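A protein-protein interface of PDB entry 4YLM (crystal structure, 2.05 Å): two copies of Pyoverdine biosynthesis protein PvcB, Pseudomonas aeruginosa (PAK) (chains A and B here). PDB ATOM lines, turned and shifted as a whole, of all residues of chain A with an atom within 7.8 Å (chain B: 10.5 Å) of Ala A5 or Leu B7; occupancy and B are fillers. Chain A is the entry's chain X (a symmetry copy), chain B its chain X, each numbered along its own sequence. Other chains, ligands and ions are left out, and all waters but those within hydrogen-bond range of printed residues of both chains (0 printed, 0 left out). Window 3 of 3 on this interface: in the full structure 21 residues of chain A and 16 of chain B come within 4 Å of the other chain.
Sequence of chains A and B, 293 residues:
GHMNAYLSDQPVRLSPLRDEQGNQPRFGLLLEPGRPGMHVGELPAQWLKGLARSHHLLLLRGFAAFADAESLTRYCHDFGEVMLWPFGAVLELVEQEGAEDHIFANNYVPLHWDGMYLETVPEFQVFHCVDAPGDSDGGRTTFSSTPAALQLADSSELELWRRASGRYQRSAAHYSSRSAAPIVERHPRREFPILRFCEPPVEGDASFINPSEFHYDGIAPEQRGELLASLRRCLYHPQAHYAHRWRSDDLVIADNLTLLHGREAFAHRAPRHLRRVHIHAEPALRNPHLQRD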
ATOM      1  N   HIS A   2      10.970 -13.744 -28.665  1.00  0.00           N
ATOM      2  CA  HIS A   2      10.652 -14.530 -27.482  1.00  0.00           C
ATOM      3  C   HIS A   2      10.200 -15.909 -27.952  1.00  0.00           C
ATOM      4  O   HIS A   2      10.018 -16.116 -29.152  1.00  0.00           O
ATOM      5  CB  HIS A   2       9.509 -13.858 -26.723  1.00  0.00           C
ATOM      6  CG  HIS A   2       8.232 -13.809 -27.500  1.00  0.00           C
ATOM      7  ND1 HIS A   2       7.979 -12.842 -28.452  1.00  0.00           N
ATOM      8  CD2 HIS A   2       7.145 -14.620 -27.489  1.00  0.00           C
ATOM      9  CE1 HIS A   2       6.787 -13.053 -28.987  1.00  0.00           C
ATOM     10  NE2 HIS A   2       6.261 -14.127 -28.422  1.00  0.00           N
ATOM     11  N   MET A   3      10.006 -16.830 -27.011  1.00  0.00           N
ATOM     12  CA  MET A   3       9.597 -18.200 -27.330  1.00  0.00           C
ATOM     13  C   MET A   3       8.142 -18.426 -26.905  1.00  0.00           C
ATOM     14  O   MET A   3       7.673 -17.823 -25.945  1.00  0.00           O
ATOM     15  CB  MET A   3      10.493 -19.206 -26.600  1.00  0.00           C
ATOM     16  CG  MET A   3      11.976 -19.164 -26.977  1.00  0.00           C
ATOM     17  SD  MET A   3      12.264 -19.620 -28.701  1.00  0.00           S
ATOM     18  CE  MET A   3      12.042 -21.408 -28.641  1.00  0.00           C
ATOM     19  N   ASN A   4       7.440 -19.335 -27.575  1.00  0.00           N
ATOM     20  CA  ASN A   4       6.050 -19.631 -27.205  1.00  0.00           C
ATOM     21  C   ASN A   4       5.815 -21.073 -26.743  1.00  0.00           C
ATOM     22  O   ASN A   4       5.913 -22.019 -27.524  1.00  0.00           O
ATOM     23  CB  ASN A   4       5.094 -19.268 -28.342  1.00  0.00           C
ATOM     24  CG  ASN A   4       3.634 -19.423 -27.954  1.00  0.00           C
ATOM     25  OD1 ASN A   4       3.306 -19.836 -26.841  1.00  0.00           O
ATOM     26  ND2 ASN A   4       2.746 -19.077 -28.876  1.00  0.00           N
ATOM     27  N   ALA A   5       5.458 -21.221 -25.474  1.00  0.00           N
ATOM     28  CA  ALA A   5       5.472 -22.513 -24.810  1.00  0.00           C
ATOM     29  C   ALA A   5       4.101 -23.162 -24.652  1.00  0.00           C
ATOM     30  O   ALA A   5       3.992 -24.235 -24.084  1.00  0.00           O
ATOM     31  CB  ALA A   5       6.147 -22.398 -23.465  1.00  0.00           C
ATOM     32  N   TYR A   6       3.057 -22.525 -25.157  1.00  0.00           N
ATOM     33  CA  TYR A   6       1.716 -23.015 -24.889  1.00  0.00           C
ATOM     34  C   TYR A   6       1.129 -23.728 -26.084  1.00  0.00           C
ATOM     35  O   TYR A   6       1.137 -23.201 -27.188  1.00  0.00           O
ATOM     36  CB  TYR A   6       0.799 -21.866 -24.495  1.00  0.00           C
ATOM     37  CG  TYR A   6       1.240 -21.164 -23.262  1.00  0.00           C
ATOM     38  CD1 TYR A   6       1.227 -21.818 -22.041  1.00  0.00           C
ATOM     39  CD2 TYR A   6       1.671 -19.843 -23.306  1.00  0.00           C
ATOM     40  CE1 TYR A   6       1.620 -21.184 -20.898  1.00  0.00           C
ATOM     41  CE2 TYR A   6       2.080 -19.200 -22.161  1.00  0.00           C
ATOM     42  CZ  TYR A   6       2.050 -19.887 -20.954  1.00  0.00           C
ATOM     43  OH  TYR A   6       2.448 -19.278 -19.795  1.00  0.00           O
ATOM     44  N   LEU A   7       0.651 -24.947 -25.848  1.00  0.00           N
ATOM     45  CA  LEU A   7      -0.192 -25.658 -26.793  1.00  0.00           C
ATOM     46  C   LEU A   7      -1.447 -26.160 -26.068  1.00  0.00           C
ATOM     47  O   LEU A   7      -1.380 -26.875 -25.044  1.00  0.00           O
ATOM     48  CB  LEU A   7       0.559 -26.789 -27.495  1.00  0.00           C
ATOM     49  CG  LEU A   7       1.000 -26.382 -28.909  1.00  0.00           C
ATOM     50  CD1 LEU A   7       1.575 -27.557 -29.682  1.00  0.00           C
ATOM     51  CD2 LEU A   7      -0.162 -25.768 -29.663  1.00  0.00           C
ATOM     52  N   SER A   8      -2.591 -25.722 -26.579  1.00  0.00           N
ATOM     53  CA  SER A   8      -3.866 -25.928 -25.912  1.00  0.00           C
ATOM     54  C   SER A   8      -4.587 -27.103 -26.531  1.00  0.00           C
ATOM     55  O   SER A   8      -4.277 -27.509 -27.650  1.00  0.00           O
ATOM     56  CB  SER A   8      -4.733 -24.677 -26.088  1.00  0.00           C
ATOM     57  OG  SER A   8      -5.869 -24.737 -25.248  1.00  0.00           O
ATOM     58  N   ASP A   9      -5.544 -27.661 -25.799  1.00  0.00           N
ATOM     59  CA  ASP A   9      -6.465 -28.611 -26.397  1.00  0.00           C
ATOM     60  C   ASP A   9      -7.718 -27.880 -26.880  1.00  0.00           C
ATOM     61  O   ASP A   9      -8.627 -28.497 -27.426  1.00  0.00           O
ATOM     62  CB  ASP A   9      -6.821 -29.734 -25.412  1.00  0.00           C
ATOM     63  CG  ASP A   9      -7.003 -29.229 -23.991  1.00  0.00           C
ATOM     64  OD1 ASP A   9      -7.168 -28.005 -23.798  1.00  0.00           O
ATOM     65  OD2 ASP A   9      -6.971 -30.059 -23.059  1.00  0.00           O
ATOM     66  N   LEU A  14      -2.371 -19.781 -28.278  1.00  0.00           N
ATOM     67  CA  LEU A  14      -1.959 -19.142 -27.046  1.00  0.00           C
ATOM     68  C   LEU A  14      -0.522 -18.637 -27.130  1.00  0.00           C
ATOM     69  O   LEU A  14       0.343 -19.267 -27.741  1.00  0.00           O
ATOM     70  CB  LEU A  14      -2.048 -20.127 -25.882  1.00  0.00           C
ATOM     71  CG  LEU A  14      -3.399 -20.762 -25.562  1.00  0.00           C
ATOM     72  CD1 LEU A  14      -3.313 -21.561 -24.276  1.00  0.00           C
ATOM     73  CD2 LEU A  14      -4.476 -19.724 -25.441  1.00  0.00           C
ATOM     74  N   SER A  15      -0.253 -17.509 -26.496  1.00  0.00           N
ATOM     75  CA  SER A  15       1.139 -17.114 -26.337  1.00  0.00           C
ATOM     76  C   SER A  15       1.322 -16.154 -25.173  1.00  0.00           C
ATOM     77  O   SER A  15       0.354 -15.571 -24.674  1.00  0.00           O
ATOM     78  CB  SER A  15       1.696 -16.547 -27.654  1.00  0.00           C
ATOM     79  OG  SER A  15       0.940 -15.463 -28.103  1.00  0.00           O
ATOM     80  N   PRO A  16       2.569 -16.006 -24.713  1.00  0.00           N
ATOM     81  CA  PRO A  16       2.847 -15.089 -23.605  1.00  0.00           C
ATOM     82  C   PRO A  16       2.356 -13.676 -23.936  1.00  0.00           C
ATOM     83  O   PRO A  16       2.436 -13.257 -25.082  1.00  0.00           O
ATOM     84  CB  PRO A  16       4.381 -15.087 -23.519  1.00  0.00           C
ATOM     85  CG  PRO A  16       4.819 -16.342 -24.201  1.00  0.00           C
ATOM     86  CD  PRO A  16       3.788 -16.644 -25.248  1.00  0.00           C
ATOM     87  N   MET B   3      10.716 -39.882 -22.417  1.00  0.00           N
ATOM     88  CA  MET B   3      10.231 -38.764 -23.231  1.00  0.00           C
ATOM     89  C   MET B   3       9.149 -37.992 -22.469  1.00  0.00           C
ATOM     90  O   MET B   3       8.420 -38.568 -21.668  1.00  0.00           O
ATOM     91  CB  MET B   3       9.643 -39.282 -24.547  1.00  0.00           C
ATOM     92  CG  MET B   3      10.625 -40.013 -25.466  1.00  0.00           C
ATOM     93  SD  MET B   3      11.942 -38.934 -26.067  1.00  0.00           S
ATOM     94  CE  MET B   3      11.070 -37.959 -27.309  1.00  0.00           C
ATOM     95  N   ASN B   4       9.000 -36.701 -22.754  1.00  0.00           N
ATOM     96  CA  ASN B   4       7.962 -35.903 -22.090  1.00  0.00           C
ATOM     97  C   ASN B   4       6.904 -35.330 -23.039  1.00  0.00           C
ATOM     98  O   ASN B   4       7.186 -34.461 -23.864  1.00  0.00           O
ATOM     99  CB  ASN B   4       8.588 -34.789 -21.248  1.00  0.00           C
ATOM    100  CG  ASN B   4       7.561 -34.025 -20.429  1.00  0.00           C
ATOM    101  OD1 ASN B   4       6.360 -34.288 -20.500  1.00  0.00           O
ATOM    102  ND2 ASN B   4       8.038 -33.075 -19.637  1.00  0.00           N
ATOM    103  N   ALA B   5       5.673 -35.799 -22.879  1.00  0.00           N
ATOM    104  CA  ALA B   5       4.626 -35.579 -23.862  1.00  0.00           C
ATOM    105  C   ALA B   5       3.623 -34.492 -23.492  1.00  0.00           C
ATOM    106  O   ALA B   5       2.686 -34.245 -24.231  1.00  0.00           O
ATOM    107  CB  ALA B   5       3.904 -36.873 -24.148  1.00  0.00           C
ATOM    108  N   TYR B   6       3.816 -33.838 -22.358  1.00  0.00           N
ATOM    109  CA  TYR B   6       2.803 -32.913 -21.878  1.00  0.00           C
ATOM    110  C   TYR B   6       3.202 -31.475 -22.105  1.00  0.00           C
ATOM    111  O   TYR B   6       4.300 -31.071 -21.745  1.00  0.00           O
ATOM    112  CB  TYR B   6       2.544 -33.129 -20.395  1.00  0.00           C
ATOM    113  CG  TYR B   6       2.045 -34.494 -20.082  1.00  0.00           C
ATOM    114  CD1 TYR B   6       0.800 -34.905 -20.533  1.00  0.00           C
ATOM    115  CD2 TYR B   6       2.809 -35.383 -19.335  1.00  0.00           C
ATOM    116  CE1 TYR B   6       0.324 -36.150 -20.248  1.00  0.00           C
ATOM    117  CE2 TYR B   6       2.341 -36.645 -19.052  1.00  0.00           C
ATOM    118  CZ  TYR B   6       1.087 -37.019 -19.518  1.00  0.00           C
ATOM    119  OH  TYR B   6       0.589 -38.266 -19.254  1.00  0.00           O
ATOM    120  N   LEU B   7       2.305 -30.721 -22.737  1.00  0.00           N
ATOM    121  CA  LEU B   7       2.393 -29.273 -22.790  1.00  0.00           C
ATOM    122  C   LEU B   7       1.049 -28.673 -22.358  1.00  0.00           C
ATOM    123  O   LEU B   7      -0.027 -28.985 -22.914  1.00  0.00           O
ATOM    124  CB  LEU B   7       2.830 -28.774 -24.167  1.00  0.00           C
ATOM    125  CG  LEU B   7       4.318 -28.398 -24.186  1.00  0.00           C
ATOM    126  CD1 LEU B   7       4.716 -27.723 -25.488  1.00  0.00           C
ATOM    127  CD2 LEU B   7       4.648 -27.508 -23.005  1.00  0.00           C
ATOM    128  N   SER B   8       1.122 -27.854 -21.315  1.00  0.00           N
ATOM    129  CA  SER B   8      -0.064 -27.351 -20.642  1.00  0.00           C
ATOM    130  C   SER B   8      -0.371 -25.950 -21.120  1.00  0.00           C
ATOM    131  O   SER B   8       0.495 -25.274 -21.674  1.00  0.00           O
ATOM    132  CB  SER B   8       0.195 -27.305 -19.133  1.00  0.00           C
ATOM    133  OG  SER B   8      -1.007 -27.065 -18.429  1.00  0.00           O
ATOM    134  N   ASP B   9      -1.609 -25.515 -20.918  1.00  0.00           N
ATOM    135  CA  ASP B   9      -1.930 -24.110 -21.095  1.00  0.00           C
ATOM    136  C   ASP B   9      -1.811 -23.383 -19.754  1.00  0.00           C
ATOM    137  O   ASP B   9      -2.033 -22.178 -19.678  1.00  0.00           O
ATOM    138  CB  ASP B   9      -3.330 -23.933 -21.700  1.00  0.00           C
ATOM    139  CG  ASP B   9      -4.339 -24.921 -21.140  1.00  0.00           C
ATOM    140  OD1 ASP B   9      -4.070 -25.528 -20.081  1.00  0.00           O
ATOM    141  OD2 ASP B   9      -5.405 -25.099 -21.766  1.00  0.00           O
ATOM    142  N   GLN B  10      -1.459 -24.126 -18.706  1.00  0.00           N
ATOM    143  CA  GLN B  10      -1.251 -23.555 -17.374  1.00  0.00           C
ATOM    144  C   GLN B  10       0.234 -23.191 -17.199  1.00  0.00           C
ATOM    145  O   GLN B  10       1.095 -23.768 -17.861  1.00  0.00           O
ATOM    146  CB  GLN B  10      -1.687 -24.557 -16.296  1.00  0.00           C
ATOM    147  CG  GLN B  10      -3.206 -24.863 -16.297  1.00  0.00           C
ATOM    148  CD  GLN B  10      -4.044 -23.695 -15.804  1.00  0.00           C
ATOM    149  OE1 GLN B  10      -3.570 -22.852 -15.036  1.00  0.00           O
ATOM    150  NE2 GLN B  10      -5.299 -23.645 -16.234  1.00  0.00           N
ATOM    151  N   PRO B  11       0.543 -22.238 -16.308  1.00  0.00           N
ATOM    152  CA  PRO B  11       1.959 -21.847 -16.124  1.00  0.00           C
ATOM    153  C   PRO B  11       2.721 -22.835 -15.240  1.00  0.00           C
ATOM    154  O   PRO B  11       3.094 -22.556 -14.085  1.00  0.00           O
ATOM    155  CB  PRO B  11       1.855 -20.458 -15.478  1.00  0.00           C
ATOM    156  CG  PRO B  11       0.577 -20.554 -14.637  1.00  0.00           C
ATOM    157  CD  PRO B  11      -0.375 -21.453 -15.457  1.00  0.00           C
ATOM    158  N   VAL B  12       2.953 -24.025 -15.791  1.00  0.00           N
ATOM    159  CA  VAL B  12       3.607 -25.108 -15.063  1.00  0.00           C
ATOM    160  C   VAL B  12       4.405 -25.963 -16.040  1.00  0.00           C
ATOM    161  O   VAL B  12       4.179 -25.898 -17.228  1.00  0.00           O
ATOM    162  CB  VAL B  12       2.589 -26.085 -14.420  1.00  0.00           C
ATOM    163  CG1 VAL B  12       1.854 -25.441 -13.285  1.00  0.00           C
ATOM    164  CG2 VAL B  12       1.619 -26.599 -15.488  1.00  0.00           C
ATOM    165  N   ARG B  13       5.334 -26.767 -15.531  1.00  0.00           N
ATOM    166  CA  ARG B  13       6.020 -27.739 -16.378  1.00  0.00           C
ATOM    167  C   ARG B  13       5.485 -29.090 -15.963  1.00  0.00           C
ATOM    168  O   ARG B  13       5.542 -29.430 -14.784  1.00  0.00           O
ATOM    169  CB  ARG B  13       7.536 -27.716 -16.143  1.00  0.00           C
ATOM    170  CG  ARG B  13       8.275 -26.576 -16.825  1.00  0.00           C
ATOM    171  CD  ARG B  13       9.692 -26.421 -16.248  1.00  0.00           C
ATOM    172  NE  ARG B  13       9.657 -25.888 -14.882  1.00  0.00           N
ATOM    173  CZ  ARG B  13      10.345 -26.380 -13.854  1.00  0.00           C
ATOM    174  NH1 ARG B  13      11.147 -27.432 -14.012  1.00  0.00           N
ATOM    175  NH2 ARG B  13      10.229 -25.811 -12.661  1.00  0.00           N
ATOM    176  N   LEU B  14       4.984 -29.859 -16.923  1.00  0.00           N
ATOM    177  CA  LEU B  14       4.446 -31.174 -16.641  1.00  0.00           C
ATOM    178  C   LEU B  14       5.362 -32.277 -17.162  1.00  0.00           C
ATOM    179  O   LEU B  14       5.981 -32.148 -18.221  1.00  0.00           O
ATOM    180  CB  LEU B  14       3.079 -31.340 -17.303  1.00  0.00           C
ATOM    181  CG  LEU B  14       1.962 -30.370 -16.927  1.00  0.00           C
ATOM    182  CD1 LEU B  14       0.652 -30.812 -17.550  1.00  0.00           C
ATOM    183  CD2 LEU B  14       1.804 -30.267 -15.438  1.00  0.00           C
ATOM    184  N   SER B  15       5.435 -33.378 -16.435  1.00  0.00           N
ATOM    185  CA  SER B  15       6.092 -34.546 -17.004  1.00  0.00           C
ATOM    186  C   SER B  15       5.636 -35.830 -16.332  1.00  0.00           C
ATOM    187  O   SER B  15       5.041 -35.804 -15.250  1.00  0.00           O
ATOM    188  CB  SER B  15       7.621 -34.380 -16.968  1.00  0.00           C
ATOM    189  OG  SER B  15       8.080 -34.158 -15.668  1.00  0.00           O
ATOM    190  N   PRO B  16       5.889 -36.968 -16.988  1.00  0.00           N
ATOM    191  CA  PRO B  16       5.503 -38.259 -16.411  1.00  0.00           C
ATOM    192  C   PRO B  16       6.119 -38.436 -15.020  1.00  0.00           C
ATOM    193  O   PRO B  16       7.238 -37.999 -14.791  1.00  0.00           O
ATOM    194  CB  PRO B  16       6.121 -39.281 -17.376  1.00  0.00           C
ATOM    195  CG  PRO B  16       6.352 -38.536 -18.650  1.00  0.00           C
ATOM    196  CD  PRO B  16       6.602 -37.106 -18.273  1.00  0.00           C
ATOM    197  N   LEU B  29       1.567 -37.960 -12.356  1.00  0.00           N
ATOM    198  CA  LEU B  29       2.021 -36.796 -13.106  1.00  0.00           C
ATOM    199  C   LEU B  29       2.838 -35.902 -12.192  1.00  0.00           C
ATOM    200  O   LEU B  29       2.487 -35.717 -11.031  1.00  0.00           O
ATOM    201  CB  LEU B  29       0.811 -36.035 -13.666  1.00  0.00           C
ATOM    202  CG  LEU B  29       1.080 -34.835 -14.581  1.00  0.00           C
ATOM    203  CD1 LEU B  29       1.608 -35.345 -15.924  1.00  0.00           C
ATOM    204  CD2 LEU B  29      -0.211 -34.029 -14.790  1.00  0.00           C
ATOM    205  N   LEU B  30       3.958 -35.387 -12.694  1.00  0.00           N
ATOM    206  CA  LEU B  30       4.779 -34.458 -11.943  1.00  0.00           C
ATOM    207  C   LEU B  30       4.478 -33.061 -12.448  1.00  0.00           C
ATOM    208  O   LEU B  30       4.504 -32.822 -13.656  1.00  0.00           O
ATOM    209  CB  LEU B  30       6.275 -34.751 -12.134  1.00  0.00           C
ATOM    210  CG  LEU B  30       7.280 -33.726 -11.582  1.00  0.00           C
ATOM    211  CD1 LEU B  30       7.190 -33.591 -10.044  1.00  0.00           C
ATOM    212  CD2 LEU B  30       8.733 -34.038 -12.002  1.00  0.00           C
ATOM    213  N   GLU B  32       5.640 -28.954 -11.940  1.00  0.00           N
ATOM    214  CA  GLU B  32       6.637 -28.076 -11.356  1.00  0.00           C
ATOM    215  C   GLU B  32       6.345 -26.641 -11.760  1.00  0.00           C
ATOM    216  O   GLU B  32       5.745 -26.395 -12.805  1.00  0.00           O
ATOM    217  CB  GLU B  32       8.046 -28.498 -11.790  1.00  0.00           C
ATOM    218  CG  GLU B  32       8.395 -29.926 -11.386  1.00  0.00           C
ATOM    219  CD  GLU B  32       9.713 -30.376 -12.001  1.00  0.00           C
ATOM    220  OE1 GLU B  32      10.742 -30.287 -11.305  1.00  0.00           O
ATOM    221  OE2 GLU B  32       9.723 -30.773 -13.193  1.00  0.00           O
ATOM    222  N   GLY B  34       5.995 -22.841 -13.016  1.00  0.00           N
ATOM    223  CA  GLY B  34       6.330 -22.184 -14.264  1.00  0.00           C
ATOM    224  C   GLY B  34       6.883 -20.779 -14.072  1.00  0.00           C
ATOM    225  O   GLY B  34       7.274 -20.134 -15.044  1.00  0.00           O
ATOM    226  N   TRP B  47      -8.885 -27.475 -12.196  1.00  0.00           N
ATOM    227  CA  TRP B  47      -7.991 -28.096 -13.157  1.00  0.00           C
ATOM    228  C   TRP B  47      -7.194 -29.245 -12.507  1.00  0.00           C
ATOM    229  O   TRP B  47      -7.060 -30.325 -13.084  1.00  0.00           O
ATOM    230  CB  TRP B  47      -7.056 -27.031 -13.722  1.00  0.00           C
ATOM    231  CG  TRP B  47      -6.023 -27.532 -14.661  1.00  0.00           C
ATOM    232  CD1 TRP B  47      -6.214 -27.969 -15.945  1.00  0.00           C
ATOM    233  CD2 TRP B  47      -4.615 -27.603 -14.415  1.00  0.00           C
ATOM    234  NE1 TRP B  47      -5.008 -28.299 -16.507  1.00  0.00           N
ATOM    235  CE2 TRP B  47      -4.013 -28.097 -15.586  1.00  0.00           C
ATOM    236  CE3 TRP B  47      -3.804 -27.285 -13.320  1.00  0.00           C
ATOM    237  CZ2 TRP B  47      -2.634 -28.291 -15.694  1.00  0.00           C
ATOM    238  CZ3 TRP B  47      -2.426 -27.479 -13.428  1.00  0.00           C
ATOM    239  CH2 TRP B  47      -1.861 -27.983 -14.612  1.00  0.00           C
ATOM    240  N   LEU B  51      -7.005 -33.368 -13.458  1.00  0.00           N
ATOM    241  CA  LEU B  51      -5.774 -34.139 -13.632  1.00  0.00           C
ATOM    242  C   LEU B  51      -5.679 -35.299 -12.633  1.00  0.00           C
ATOM    243  O   LEU B  51      -5.249 -36.390 -12.994  1.00  0.00           O
ATOM    244  CB  LEU B  51      -4.538 -33.243 -13.494  1.00  0.00           C
ATOM    245  CG  LEU B  51      -4.362 -32.120 -14.526  1.00  0.00           C
ATOM    246  CD1 LEU B  51      -3.168 -31.235 -14.158  1.00  0.00           C
ATOM    247  CD2 LEU B  51      -4.236 -32.684 -15.946  1.00  0.00           C
ATOM    248  N   HIS B  55      -4.980 -38.944 -14.077  1.00  0.00           N
ATOM    249  CA  HIS B  55      -3.625 -39.405 -13.815  1.00  0.00           C
ATOM    250  C   HIS B  55      -3.527 -40.117 -12.456  1.00  0.00           C
ATOM    251  O   HIS B  55      -2.529 -40.778 -12.184  1.00  0.00           O
ATOM    252  CB  HIS B  55      -2.641 -38.238 -13.832  1.00  0.00           C
ATOM    253  CG  HIS B  55      -2.501 -37.566 -15.168  1.00  0.00           C
ATOM    254  ND1 HIS B  55      -1.712 -38.073 -16.179  1.00  0.00           N
ATOM    255  CD2 HIS B  55      -3.014 -36.403 -15.640  1.00  0.00           C
ATOM    256  CE1 HIS B  55      -1.755 -37.259 -17.219  1.00  0.00           C
ATOM    257  NE2 HIS B  55      -2.547 -36.243 -16.922  1.00  0.00           N
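Ala A5 touches one residue of chain B. Printed residues of chain B within 4 Å of Leu A7: Leu B7 (3.3 Å). Printed residues of chain B within 4 Å of Asp A9: Asp B9. Of the printed residues of chain A, Ser B8 touches Tyr A6 (3.6 Å). Printed residues of chain A within 4 Å of Asp B9: Tyr A6 (3.98 Å), Ser A8 (3.5 Å), Asp A9 (3.96 Å) and Leu A14 (3.5 Å). Ser A15 touches none of the printed residues of chain B. The nearest residue of chain B that does not touch Ala A5 is Ser B8 (4.4 Å). The nearest residue of chain A that does not touch Leu B7 is Tyr A6 (5.4 Å).
OD1 of Asn A4 is in hydrogen-bond range of N of Tyr A6 (3.2 Å). N of Gln B10 lies within hydrogen-bond range of OG of Ser B8 (3.0 Å). ND2 of Asn A4 lies within hydrogen-bond range of O of Leu A14, 2.7 Å away.
Leu B7 touches Ala A5. Ser B8 touches Tyr A6. Tyr A6 touches Asp B9. OG of Ser A8 touches OD2 of Asp B9, at 3.5 Å. OD2 of Asp B9 touches OD1 of Asp A9 (3.96 Å). CB of Asp B9 touches CD1 of Leu A14, at 3.5 Å.
Of the 21 printed residues of chain B, 3 touch a printed residue of chain A. Hydrophobic or aromatic side chains of chain B within 4 Å of the printed part of chain A: Leu B7. Among the printed residues, 7 pairs touch across the chains.
The backbone carbonyl oxygen of Leu A7 sits close to the backbone carbonyl oxygen of Leu B7 (3.3 Å).
Ala A5 touches Leu B7, but with the chains exchanged Leu A7 does not touch Ala B5 (8.4 Å). Tyr A6 touches Asp B9, but with the chains exchanged Asp A9 does not touch Tyr B6 (9.5 Å). Ser A8 touches Asp B9, but with the chains exchanged Asp A9 does not touch Ser B8 (7.2 Å). Asp B9 touches its own counterpart, Asp A9. Of the 7 pairs that touch across the chains among the printed residues, 2 have their exchanged pair printed and touching as well.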
